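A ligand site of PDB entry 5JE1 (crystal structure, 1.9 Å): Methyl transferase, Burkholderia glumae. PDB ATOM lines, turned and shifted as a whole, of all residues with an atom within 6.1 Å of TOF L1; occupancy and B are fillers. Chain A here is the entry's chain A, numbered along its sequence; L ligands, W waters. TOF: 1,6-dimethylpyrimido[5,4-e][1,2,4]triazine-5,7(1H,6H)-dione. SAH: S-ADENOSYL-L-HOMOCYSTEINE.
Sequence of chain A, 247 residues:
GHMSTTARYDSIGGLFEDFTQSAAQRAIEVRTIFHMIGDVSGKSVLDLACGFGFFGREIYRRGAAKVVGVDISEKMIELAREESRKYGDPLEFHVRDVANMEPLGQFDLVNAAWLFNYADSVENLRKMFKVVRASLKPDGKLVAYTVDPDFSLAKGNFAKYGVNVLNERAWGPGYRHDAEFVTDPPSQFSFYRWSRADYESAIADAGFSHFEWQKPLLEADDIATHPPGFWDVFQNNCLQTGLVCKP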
ATOM      1  N   TYR A   9      10.549  31.458  -3.732  1.00  0.00           N
ATOM      2  CA  TYR A   9       9.349  30.715  -3.350  1.00  0.00           C
ATOM      3  C   TYR A   9       9.213  30.517  -1.855  1.00  0.00           C
ATOM      4  O   TYR A   9       8.192  29.986  -1.417  1.00  0.00           O
ATOM      5  CB  TYR A   9       9.330  29.360  -4.041  1.00  0.00           C
ATOM      6  CG  TYR A   9       8.721  29.449  -5.422  1.00  0.00           C
ATOM      7  CD1 TYR A   9       7.483  28.884  -5.689  1.00  0.00           C
ATOM      8  CD2 TYR A   9       9.381  30.131  -6.443  1.00  0.00           C
ATOM      9  CE1 TYR A   9       6.934  28.971  -6.970  1.00  0.00           C
ATOM     10  CE2 TYR A   9       8.837  30.226  -7.708  1.00  0.00           C
ATOM     11  CZ  TYR A   9       7.612  29.647  -7.960  1.00  0.00           C
ATOM     12  OH  TYR A   9       7.097  29.729  -9.228  1.00  0.00           O
ATOM     13  N   PHE A  16       1.519  28.185  -4.077  1.00  0.00           N
ATOM     14  CA  PHE A  16       1.727  27.572  -5.383  1.00  0.00           C
ATOM     15  C   PHE A  16       0.764  26.412  -5.583  1.00  0.00           C
ATOM     16  O   PHE A  16       0.194  26.250  -6.672  1.00  0.00           O
ATOM     17  CB  PHE A  16       3.165  27.098  -5.559  1.00  0.00           C
ATOM     18  CG  PHE A  16       3.402  26.465  -6.900  1.00  0.00           C
ATOM     19  CD1 PHE A  16       3.327  27.257  -8.052  1.00  0.00           C
ATOM     20  CD2 PHE A  16       3.619  25.105  -7.017  1.00  0.00           C
ATOM     21  CE1 PHE A  16       3.510  26.684  -9.286  1.00  0.00           C
ATOM     22  CE2 PHE A  16       3.796  24.523  -8.267  1.00  0.00           C
ATOM     23  CZ  PHE A  16       3.746  25.312  -9.403  1.00  0.00           C
ATOM     24  N   PHE A  19      -2.482  27.716  -6.595  1.00  0.00           N
ATOM     25  CA  PHE A  19      -2.471  28.038  -8.014  1.00  0.00           C
ATOM     26  C   PHE A  19      -2.687  26.789  -8.869  1.00  0.00           C
ATOM     27  O   PHE A  19      -3.433  26.838  -9.852  1.00  0.00           O
ATOM     28  CB  PHE A  19      -1.162  28.728  -8.385  1.00  0.00           C
ATOM     29  CG  PHE A  19      -0.755  28.539  -9.806  1.00  0.00           C
ATOM     30  CD1 PHE A  19      -1.290  29.353 -10.808  1.00  0.00           C
ATOM     31  CD2 PHE A  19       0.157  27.556 -10.153  1.00  0.00           C
ATOM     32  CE1 PHE A  19      -0.893  29.195 -12.133  1.00  0.00           C
ATOM     33  CE2 PHE A  19       0.541  27.378 -11.475  1.00  0.00           C
ATOM     34  CZ  PHE A  19       0.006  28.191 -12.476  1.00  0.00           C
ATOM     35  N   GLN A  25      -4.459  26.734 -16.992  1.00  0.00           N
ATOM     36  CA  GLN A  25      -3.336  26.200 -17.761  1.00  0.00           C
ATOM     37  C   GLN A  25      -2.722  24.938 -17.133  1.00  0.00           C
ATOM     38  O   GLN A  25      -2.013  24.209 -17.831  1.00  0.00           O
ATOM     39  CB  GLN A  25      -2.239  27.254 -17.915  1.00  0.00           C
ATOM     40  CG  GLN A  25      -1.480  27.521 -16.630  1.00  0.00           C
ATOM     41  CD  GLN A  25      -0.255  28.387 -16.849  1.00  0.00           C
ATOM     42  OE1 GLN A  25      -0.359  29.519 -17.347  1.00  0.00           O
ATOM     43  NE2 GLN A  25       0.917  27.871 -16.492  1.00  0.00           N
ATOM     44  N   ARG A  26      -2.968  24.685 -15.843  1.00  0.00           N
ATOM     45  CA  ARG A  26      -2.266  23.599 -15.164  1.00  0.00           C
ATOM     46  C   ARG A  26      -2.593  22.250 -15.790  1.00  0.00           C
ATOM     47  O   ARG A  26      -1.692  21.426 -16.015  1.00  0.00           O
ATOM     48  CB  ARG A  26      -2.590  23.598 -13.670  1.00  0.00           C
ATOM     49  CG  ARG A  26      -1.861  22.525 -12.864  1.00  0.00           C
ATOM     50  CD  ARG A  26      -0.321  22.719 -12.905  1.00  0.00           C
ATOM     51  NE  ARG A  26       0.342  21.828 -11.958  1.00  0.00           N
ATOM     52  CZ  ARG A  26       1.656  21.814 -11.703  1.00  0.00           C
ATOM     53  NH1 ARG A  26       2.469  22.660 -12.320  1.00  0.00           N
ATOM     54  NH2 ARG A  26       2.153  20.963 -10.811  1.00  0.00           N
ATOM     55  N   GLU A  29      -0.483  21.770 -18.827  1.00  0.00           N
ATOM     56  CA  GLU A  29       0.906  21.451 -18.457  1.00  0.00           C
ATOM     57  C   GLU A  29       1.058  19.992 -18.074  1.00  0.00           C
ATOM     58  O   GLU A  29       1.955  19.283 -18.565  1.00  0.00           O
ATOM     59  CB  GLU A  29       1.359  22.308 -17.272  1.00  0.00           C
ATOM     60  CG  GLU A  29       1.186  23.797 -17.375  1.00  0.00           C
ATOM     61  CD  GLU A  29       1.412  24.481 -16.033  1.00  0.00           C
ATOM     62  OE1 GLU A  29       2.232  23.984 -15.217  1.00  0.00           O
ATOM     63  OE2 GLU A  29       0.751  25.514 -15.796  1.00  0.00           O
ATOM     64  N   ALA A 113      10.248  20.618 -14.784  1.00  0.00           N
ATOM     65  CA  ALA A 113       9.089  21.460 -15.071  1.00  0.00           C
ATOM     66  C   ALA A 113       9.279  22.799 -14.364  1.00  0.00           C
ATOM     67  O   ALA A 113       9.283  22.866 -13.128  1.00  0.00           O
ATOM     68  CB  ALA A 113       7.804  20.771 -14.615  1.00  0.00           C
ATOM     69  N   TRP A 114       9.428  23.869 -15.152  1.00  0.00           N
ATOM     70  CA  TRP A 114       9.588  25.227 -14.637  1.00  0.00           C
ATOM     71  C   TRP A 114      10.900  25.412 -13.877  1.00  0.00           C
ATOM     72  O   TRP A 114      10.943  26.013 -12.793  1.00  0.00           O
ATOM     73  CB  TRP A 114       8.397  25.651 -13.781  1.00  0.00           C
ATOM     74  CG  TRP A 114       7.102  25.541 -14.528  1.00  0.00           C
ATOM     75  CD1 TRP A 114       6.085  24.676 -14.280  1.00  0.00           C
ATOM     76  CD2 TRP A 114       6.701  26.321 -15.670  1.00  0.00           C
ATOM     77  NE1 TRP A 114       5.072  24.867 -15.179  1.00  0.00           N
ATOM     78  CE2 TRP A 114       5.421  25.869 -16.043  1.00  0.00           C
ATOM     79  CE3 TRP A 114       7.293  27.357 -16.403  1.00  0.00           C
ATOM     80  CZ2 TRP A 114       4.716  26.428 -17.116  1.00  0.00           C
ATOM     81  CZ3 TRP A 114       6.595  27.901 -17.483  1.00  0.00           C
ATOM     82  CH2 TRP A 114       5.324  27.437 -17.817  1.00  0.00           C
ATOM     83  N   ASN A 117      13.394  28.578 -16.886  1.00  0.00           N
ATOM     84  CA  ASN A 117      12.935  29.972 -16.901  1.00  0.00           C
ATOM     85  C   ASN A 117      13.329  30.725 -15.636  1.00  0.00           C
ATOM     86  O   ASN A 117      13.028  31.930 -15.535  1.00  0.00           O
ATOM     87  CB  ASN A 117      11.421  30.004 -17.090  1.00  0.00           C
ATOM     88  CG  ASN A 117      10.703  29.146 -16.058  1.00  0.00           C
ATOM     89  OD1 ASN A 117      10.882  27.928 -16.022  1.00  0.00           O
ATOM     90  ND2 ASN A 117       9.919  29.784 -15.197  1.00  0.00           N
ATOM     91  N   TYR A 118      13.979  30.063 -14.689  1.00  0.00           N
ATOM     92  CA  TYR A 118      14.513  30.739 -13.520  1.00  0.00           C
ATOM     93  C   TYR A 118      16.033  30.886 -13.564  1.00  0.00           C
ATOM     94  O   TYR A 118      16.617  31.444 -12.625  1.00  0.00           O
ATOM     95  CB  TYR A 118      14.066  30.004 -12.237  1.00  0.00           C
ATOM     96  CG  TYR A 118      12.557  30.115 -12.015  1.00  0.00           C
ATOM     97  CD1 TYR A 118      11.970  31.325 -11.664  1.00  0.00           C
ATOM     98  CD2 TYR A 118      11.730  29.017 -12.181  1.00  0.00           C
ATOM     99  CE1 TYR A 118      10.591  31.433 -11.464  1.00  0.00           C
ATOM    100  CE2 TYR A 118      10.345  29.107 -11.993  1.00  0.00           C
ATOM    101  CZ  TYR A 118       9.777  30.305 -11.643  1.00  0.00           C
ATOM    102  OH  TYR A 118       8.410  30.375 -11.451  1.00  0.00           O
ATOM    103  N   VAL A 147       9.234  28.505 -20.427  1.00  0.00           N
ATOM    104  CA  VAL A 147       8.625  29.636 -21.105  1.00  0.00           C
ATOM    105  C   VAL A 147       8.909  29.525 -22.595  1.00  0.00           C
ATOM    106  O   VAL A 147      10.038  29.234 -23.007  1.00  0.00           O
ATOM    107  CB  VAL A 147       9.160  30.947 -20.501  1.00  0.00           C
ATOM    108  CG1 VAL A 147       8.755  32.163 -21.328  1.00  0.00           C
ATOM    109  CG2 VAL A 147       8.670  31.095 -19.051  1.00  0.00           C
ATOM    110  N   PHE A 158      -1.595  36.487 -19.767  1.00  0.00           N
ATOM    111  CA  PHE A 158      -1.983  35.131 -19.417  1.00  0.00           C
ATOM    112  C   PHE A 158      -2.783  35.040 -18.138  1.00  0.00           C
ATOM    113  O   PHE A 158      -2.957  33.936 -17.598  1.00  0.00           O
ATOM    114  CB  PHE A 158      -0.725  34.260 -19.284  1.00  0.00           C
ATOM    115  CG  PHE A 158      -0.663  33.154 -20.286  1.00  0.00           C
ATOM    116  CD1 PHE A 158      -0.604  31.829 -19.869  1.00  0.00           C
ATOM    117  CD2 PHE A 158      -0.654  33.430 -21.644  1.00  0.00           C
ATOM    118  CE1 PHE A 158      -0.539  30.809 -20.800  1.00  0.00           C
ATOM    119  CE2 PHE A 158      -0.601  32.398 -22.575  1.00  0.00           C
ATOM    120  CZ  PHE A 158      -0.536  31.091 -22.147  1.00  0.00           C
ATOM    121  N   VAL A 163      -1.681  32.996 -14.764  1.00  0.00           N
ATOM    122  CA  VAL A 163      -0.410  33.700 -14.575  1.00  0.00           C
ATOM    123  C   VAL A 163      -0.546  35.125 -15.102  1.00  0.00           C
ATOM    124  O   VAL A 163      -0.601  35.343 -16.318  1.00  0.00           O
ATOM    125  CB  VAL A 163       0.764  32.983 -15.239  1.00  0.00           C
ATOM    126  CG1 VAL A 163       2.072  33.696 -14.888  1.00  0.00           C
ATOM    127  CG2 VAL A 163       0.817  31.516 -14.790  1.00  0.00           C
ATOM    128  N   VAL A 165       1.126  38.216 -16.063  1.00  0.00           N
ATOM    129  CA  VAL A 165       2.440  38.729 -16.422  1.00  0.00           C
ATOM    130  C   VAL A 165       2.374  40.254 -16.356  1.00  0.00           C
ATOM    131  O   VAL A 165       1.615  40.877 -17.108  1.00  0.00           O
ATOM    132  CB  VAL A 165       2.866  38.236 -17.815  1.00  0.00           C
ATOM    133  CG1 VAL A 165       4.234  38.759 -18.176  1.00  0.00           C
ATOM    134  CG2 VAL A 165       2.859  36.697 -17.869  1.00  0.00           C
ATOM    135  N   PHE A 181       1.106  34.616  -9.689  1.00  0.00           N
ATOM    136  CA  PHE A 181       0.093  33.575  -9.840  1.00  0.00           C
ATOM    137  C   PHE A 181      -1.233  34.110  -9.343  1.00  0.00           C
ATOM    138  O   PHE A 181      -1.296  34.814  -8.323  1.00  0.00           O
ATOM    139  CB  PHE A 181       0.469  32.315  -9.050  1.00  0.00           C
ATOM    140  CG  PHE A 181       1.746  31.667  -9.503  1.00  0.00           C
ATOM    141  CD1 PHE A 181       1.851  31.132 -10.775  1.00  0.00           C
ATOM    142  CD2 PHE A 181       2.817  31.543  -8.626  1.00  0.00           C
ATOM    143  CE1 PHE A 181       3.030  30.511 -11.182  1.00  0.00           C
ATOM    144  CE2 PHE A 181       3.981  30.931  -9.019  1.00  0.00           C
ATOM    145  CZ  PHE A 181       4.098  30.415 -10.296  1.00  0.00           C
ATOM    146  N   PHE A 189       6.345  36.729  -8.484  1.00  0.00           N
ATOM    147  CA  PHE A 189       7.589  36.060  -8.852  1.00  0.00           C
ATOM    148  C   PHE A 189       8.083  36.701 -10.137  1.00  0.00           C
ATOM    149  O   PHE A 189       7.375  37.492 -10.772  1.00  0.00           O
ATOM    150  CB  PHE A 189       7.406  34.532  -9.014  1.00  0.00           C
ATOM    151  CG  PHE A 189       6.563  34.120 -10.211  1.00  0.00           C
ATOM    152  CD1 PHE A 189       7.160  33.585 -11.346  1.00  0.00           C
ATOM    153  CD2 PHE A 189       5.188  34.252 -10.195  1.00  0.00           C
ATOM    154  CE1 PHE A 189       6.410  33.175 -12.435  1.00  0.00           C
ATOM    155  CE2 PHE A 189       4.401  33.850 -11.311  1.00  0.00           C
ATOM    156  CZ  PHE A 189       5.026  33.326 -12.426  1.00  0.00           C
ATOM    157  N   SER A 190       9.318  36.392 -10.496  1.00  0.00           N
ATOM    158  CA  SER A 190       9.902  36.872 -11.738  1.00  0.00           C
ATOM    159  C   SER A 190      10.495  35.691 -12.492  1.00  0.00           C
ATOM    160  O   SER A 190      10.920  34.698 -11.879  1.00  0.00           O
ATOM    161  CB  SER A 190      10.986  37.929 -11.455  1.00  0.00           C
ATOM    162  OG  SER A 190      10.480  39.004 -10.664  1.00  0.00           O
ATOM    163  N   PHE A 191      10.528  35.793 -13.811  1.00  0.00           N
ATOM    164  CA  PHE A 191      11.066  34.719 -14.640  1.00  0.00           C
ATOM    165  C   PHE A 191      11.745  35.332 -15.847  1.00  0.00           C
ATOM    166  O   PHE A 191      11.605  36.524 -16.136  1.00  0.00           O
ATOM    167  CB  PHE A 191       9.976  33.720 -15.048  1.00  0.00           C
ATOM    168  CG  PHE A 191       8.898  34.283 -15.958  1.00  0.00           C
ATOM    169  CD1 PHE A 191       9.027  34.216 -17.353  1.00  0.00           C
ATOM    170  CD2 PHE A 191       7.730  34.823 -15.428  1.00  0.00           C
ATOM    171  CE1 PHE A 191       8.017  34.709 -18.203  1.00  0.00           C
ATOM    172  CE2 PHE A 191       6.726  35.325 -16.261  1.00  0.00           C
ATOM    173  CZ  PHE A 191       6.868  35.261 -17.650  1.00  0.00           C
ATOM    174  N   LEU A 239       2.494  31.161 -23.466  1.00  0.00           N
ATOM    175  CA  LEU A 239       3.569  31.430 -22.519  1.00  0.00           C
ATOM    176  C   LEU A 239       4.446  30.208 -22.288  1.00  0.00           C
ATOM    177  O   LEU A 239       5.608  30.357 -21.885  1.00  0.00           O
ATOM    178  CB  LEU A 239       2.954  31.904 -21.187  1.00  0.00           C
ATOM    179  CG  LEU A 239       3.887  32.369 -20.077  1.00  0.00           C
ATOM    180  CD1 LEU A 239       4.892  33.386 -20.608  1.00  0.00           C
ATOM    181  CD2 LEU A 239       3.111  32.961 -18.906  1.00  0.00           C
ATOM    182  N   GLN A 240       3.951  29.002 -22.556  1.00  0.00           N
ATOM    183  CA  GLN A 240       4.634  27.790 -22.125  1.00  0.00           C
ATOM    184  C   GLN A 240       4.942  26.880 -23.305  1.00  0.00           C
ATOM    185  O   GLN A 240       4.295  26.936 -24.353  1.00  0.00           O
ATOM    186  CB  GLN A 240       3.793  27.056 -21.079  1.00  0.00           C
ATOM    187  CG  GLN A 240       2.364  26.800 -21.538  1.00  0.00           C
ATOM    188  CD  GLN A 240       1.555  26.009 -20.532  1.00  0.00           C
ATOM    189  OE1 GLN A 240       1.202  24.851 -20.773  1.00  0.00           O
ATOM    190  NE2 GLN A 240       1.272  26.619 -19.378  1.00  0.00           N
HETATM  191  C1  TOF L   1       4.543  30.020 -15.717  1.00  0.00           C
HETATM  192  O1  TOF L   1       3.720  30.242 -16.597  1.00  0.00           O
HETATM  193  C2  TOF L   1       4.351  28.981 -14.689  1.00  0.00           C
HETATM  194  O2  TOF L   1       7.602  31.142 -14.644  1.00  0.00           O
HETATM  195  N3  TOF L   1       3.286  28.215 -14.634  1.00  0.00           N
HETATM  196  C4  TOF L   1       3.177  27.294 -13.678  1.00  0.00           C
HETATM  197  N5  TOF L   1       4.112  27.129 -12.776  1.00  0.00           N
HETATM  198  N6  TOF L   1       5.176  27.849 -12.769  1.00  0.00           N
HETATM  199  C7  TOF L   1       5.360  28.805 -13.701  1.00  0.00           C
HETATM  200  N8  TOF L   1       6.453  29.547 -13.717  1.00  0.00           N
HETATM  201  C9  TOF L   1       6.599  30.476 -14.655  1.00  0.00           C
HETATM  202  N10 TOF L   1       5.701  30.726 -15.630  1.00  0.00           N
HETATM  203  C11 TOF L   1       6.200  27.655 -11.753  1.00  0.00           C
HETATM  204  C12 TOF L   1       5.963  31.780 -16.609  1.00  0.00           C
HETATM  205  N   SAH L   2       7.976  21.594 -10.840  1.00  0.00           N
HETATM  206  CA  SAH L   2       6.941  21.932  -9.864  1.00  0.00           C
HETATM  207  CB  SAH L   2       7.195  23.288  -9.166  1.00  0.00           C
HETATM  208  CG  SAH L   2       7.451  24.441 -10.113  1.00  0.00           C
HETATM  209  SD  SAH L   2       7.492  25.961  -9.184  1.00  0.00           S
HETATM  210  C   SAH L   2       5.537  21.861 -10.423  1.00  0.00           C
HETATM  211  O   SAH L   2       4.641  21.394  -9.659  1.00  0.00           O
HETATM  212  OXT SAH L   2       5.275  22.268 -11.593  1.00  0.00           O
HETATM  213  C5' SAH L   2       9.099  26.529  -9.624  1.00  0.00           C
HETATM  214  C4' SAH L   2      10.082  25.993  -8.584  1.00  0.00           C
HETATM  215  O4' SAH L   2      11.427  26.110  -9.038  1.00  0.00           O
HETATM  216  C3' SAH L   2      10.029  26.690  -7.228  1.00  0.00           C
HETATM  217  O3' SAH L   2       9.821  25.693  -6.205  1.00  0.00           O
HETATM  218  C2' SAH L   2      11.407  27.321  -7.063  1.00  0.00           C
HETATM  219  O2' SAH L   2      11.872  27.348  -5.703  1.00  0.00           O
HETATM  220  C1' SAH L   2      12.260  26.401  -7.915  1.00  0.00           C
HETATM  221  N9  SAH L   2      13.510  27.002  -8.406  1.00  0.00           N
HETATM  222  C8  SAH L   2      13.663  28.248  -8.920  1.00  0.00           C
HETATM  223  N7  SAH L   2      14.961  28.437  -9.287  1.00  0.00           N
HETATM  224  C5  SAH L   2      15.617  27.291  -9.027  1.00  0.00           C
HETATM  225  C6  SAH L   2      17.005  26.827  -9.166  1.00  0.00           C
HETATM  226  N6  SAH L   2      17.932  27.672  -9.681  1.00  0.00           N
HETATM  227  N1  SAH L   2      17.302  25.568  -8.768  1.00  0.00           N
HETATM  228  C2  SAH L   2      16.369  24.739  -8.247  1.00  0.00           C
HETATM  229  N3  SAH L   2      15.078  25.112  -8.083  1.00  0.00           N
HETATM  230  C4  SAH L   2      14.661  26.355  -8.451  1.00  0.00           C
HETATM  231  O   HOH W   1       2.343  29.203 -18.547  1.00  0.00           O
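NE1 of Trp 114 sits close to N5 of TOF L1 (3.4 Å).
The guanidinium group (NH2) of Arg 26 lies within salt-bridge range of an oxygen (O) of SAH L2 (2.8 Å).
A nitrogen (N) of SAH L2 sits at hydrogen-bond distance from the backbone carbonyl oxygen of Ala 113 (2.9 Å).
The side-chain hydroxyl (OH) of Tyr 118 sits at hydrogen-bond distance from a nitrogen (N8) of TOF L1.
A sulfur (SD) of SAH L2 sits close to the side-chain hydroxyl of Tyr 9, 3.8 Å away.
The side-chain amide nitrogen (ND2) of Asn 117 is in hydrogen-bond range of an oxygen (O2) of TOF L1, 2.7 Å away.
A nitrogen (N3) of TOF L1 sits at hydrogen-bond distance from the side-chain amide nitrogen of Gln 25 (3.0 Å).
The side-chain amide nitrogen (NE2) of Gln 25 sits close to the side-chain amide nitrogen (NE2) of Gln 240 (3.2 Å).
The side-chain hydroxyl (OH) of Tyr 118 lies within hydrogen-bond range of the side-chain hydroxyl (OH) of Tyr 9 (2.7 Å).
The backbone NH (N) of Val 163 sits at hydrogen-bond distance from the backbone carbonyl oxygen (O) of Phe 158.
OE1 of Glu 29 lies within hydrogen-bond range of NE1 of Trp 114 (3.0 Å).
NE2 of Gln 25 is in hydrogen-bond range of OE2 of Glu 29 (2.5 Å).
NH1 of Arg 26 lies within salt-bridge range of OE1 of Glu 29.
Merely in contact with TOF L1: Tyr 9 (3.4 Å), Phe 16 (3.6 Å), Phe 19 (3.4 Å), Glu 29 (3.7 Å), Val 147 (3.7 Å), Val 163 (3.6 Å), Phe 181 (3.7 Å), Phe 189 (3.2 Å), Phe 191 (3.5 Å) and Leu 239 (3.6 Å).
Hydrophobic or aromatic side chains within 4 Å of TOF L1: Phe 16, Phe 19, Trp 114, Tyr 118, Val 147, Val 163, Phe 181, Phe 189, Phe 191 and Leu 239.
Of the 20 residues printed, 14 come within 4 Å of TOF L1.
Along chain A the residues within 4 Å of TOF L1 span positions 9 to 239.
Water W1 lies within hydrogen-bond range of an oxygen (O1) of TOF L1 (2.6 Å), the side-chain amide nitrogen of Gln 25 (2.8 Å) and the side-chain amide nitrogen of Gln 240 (2.9 Å).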
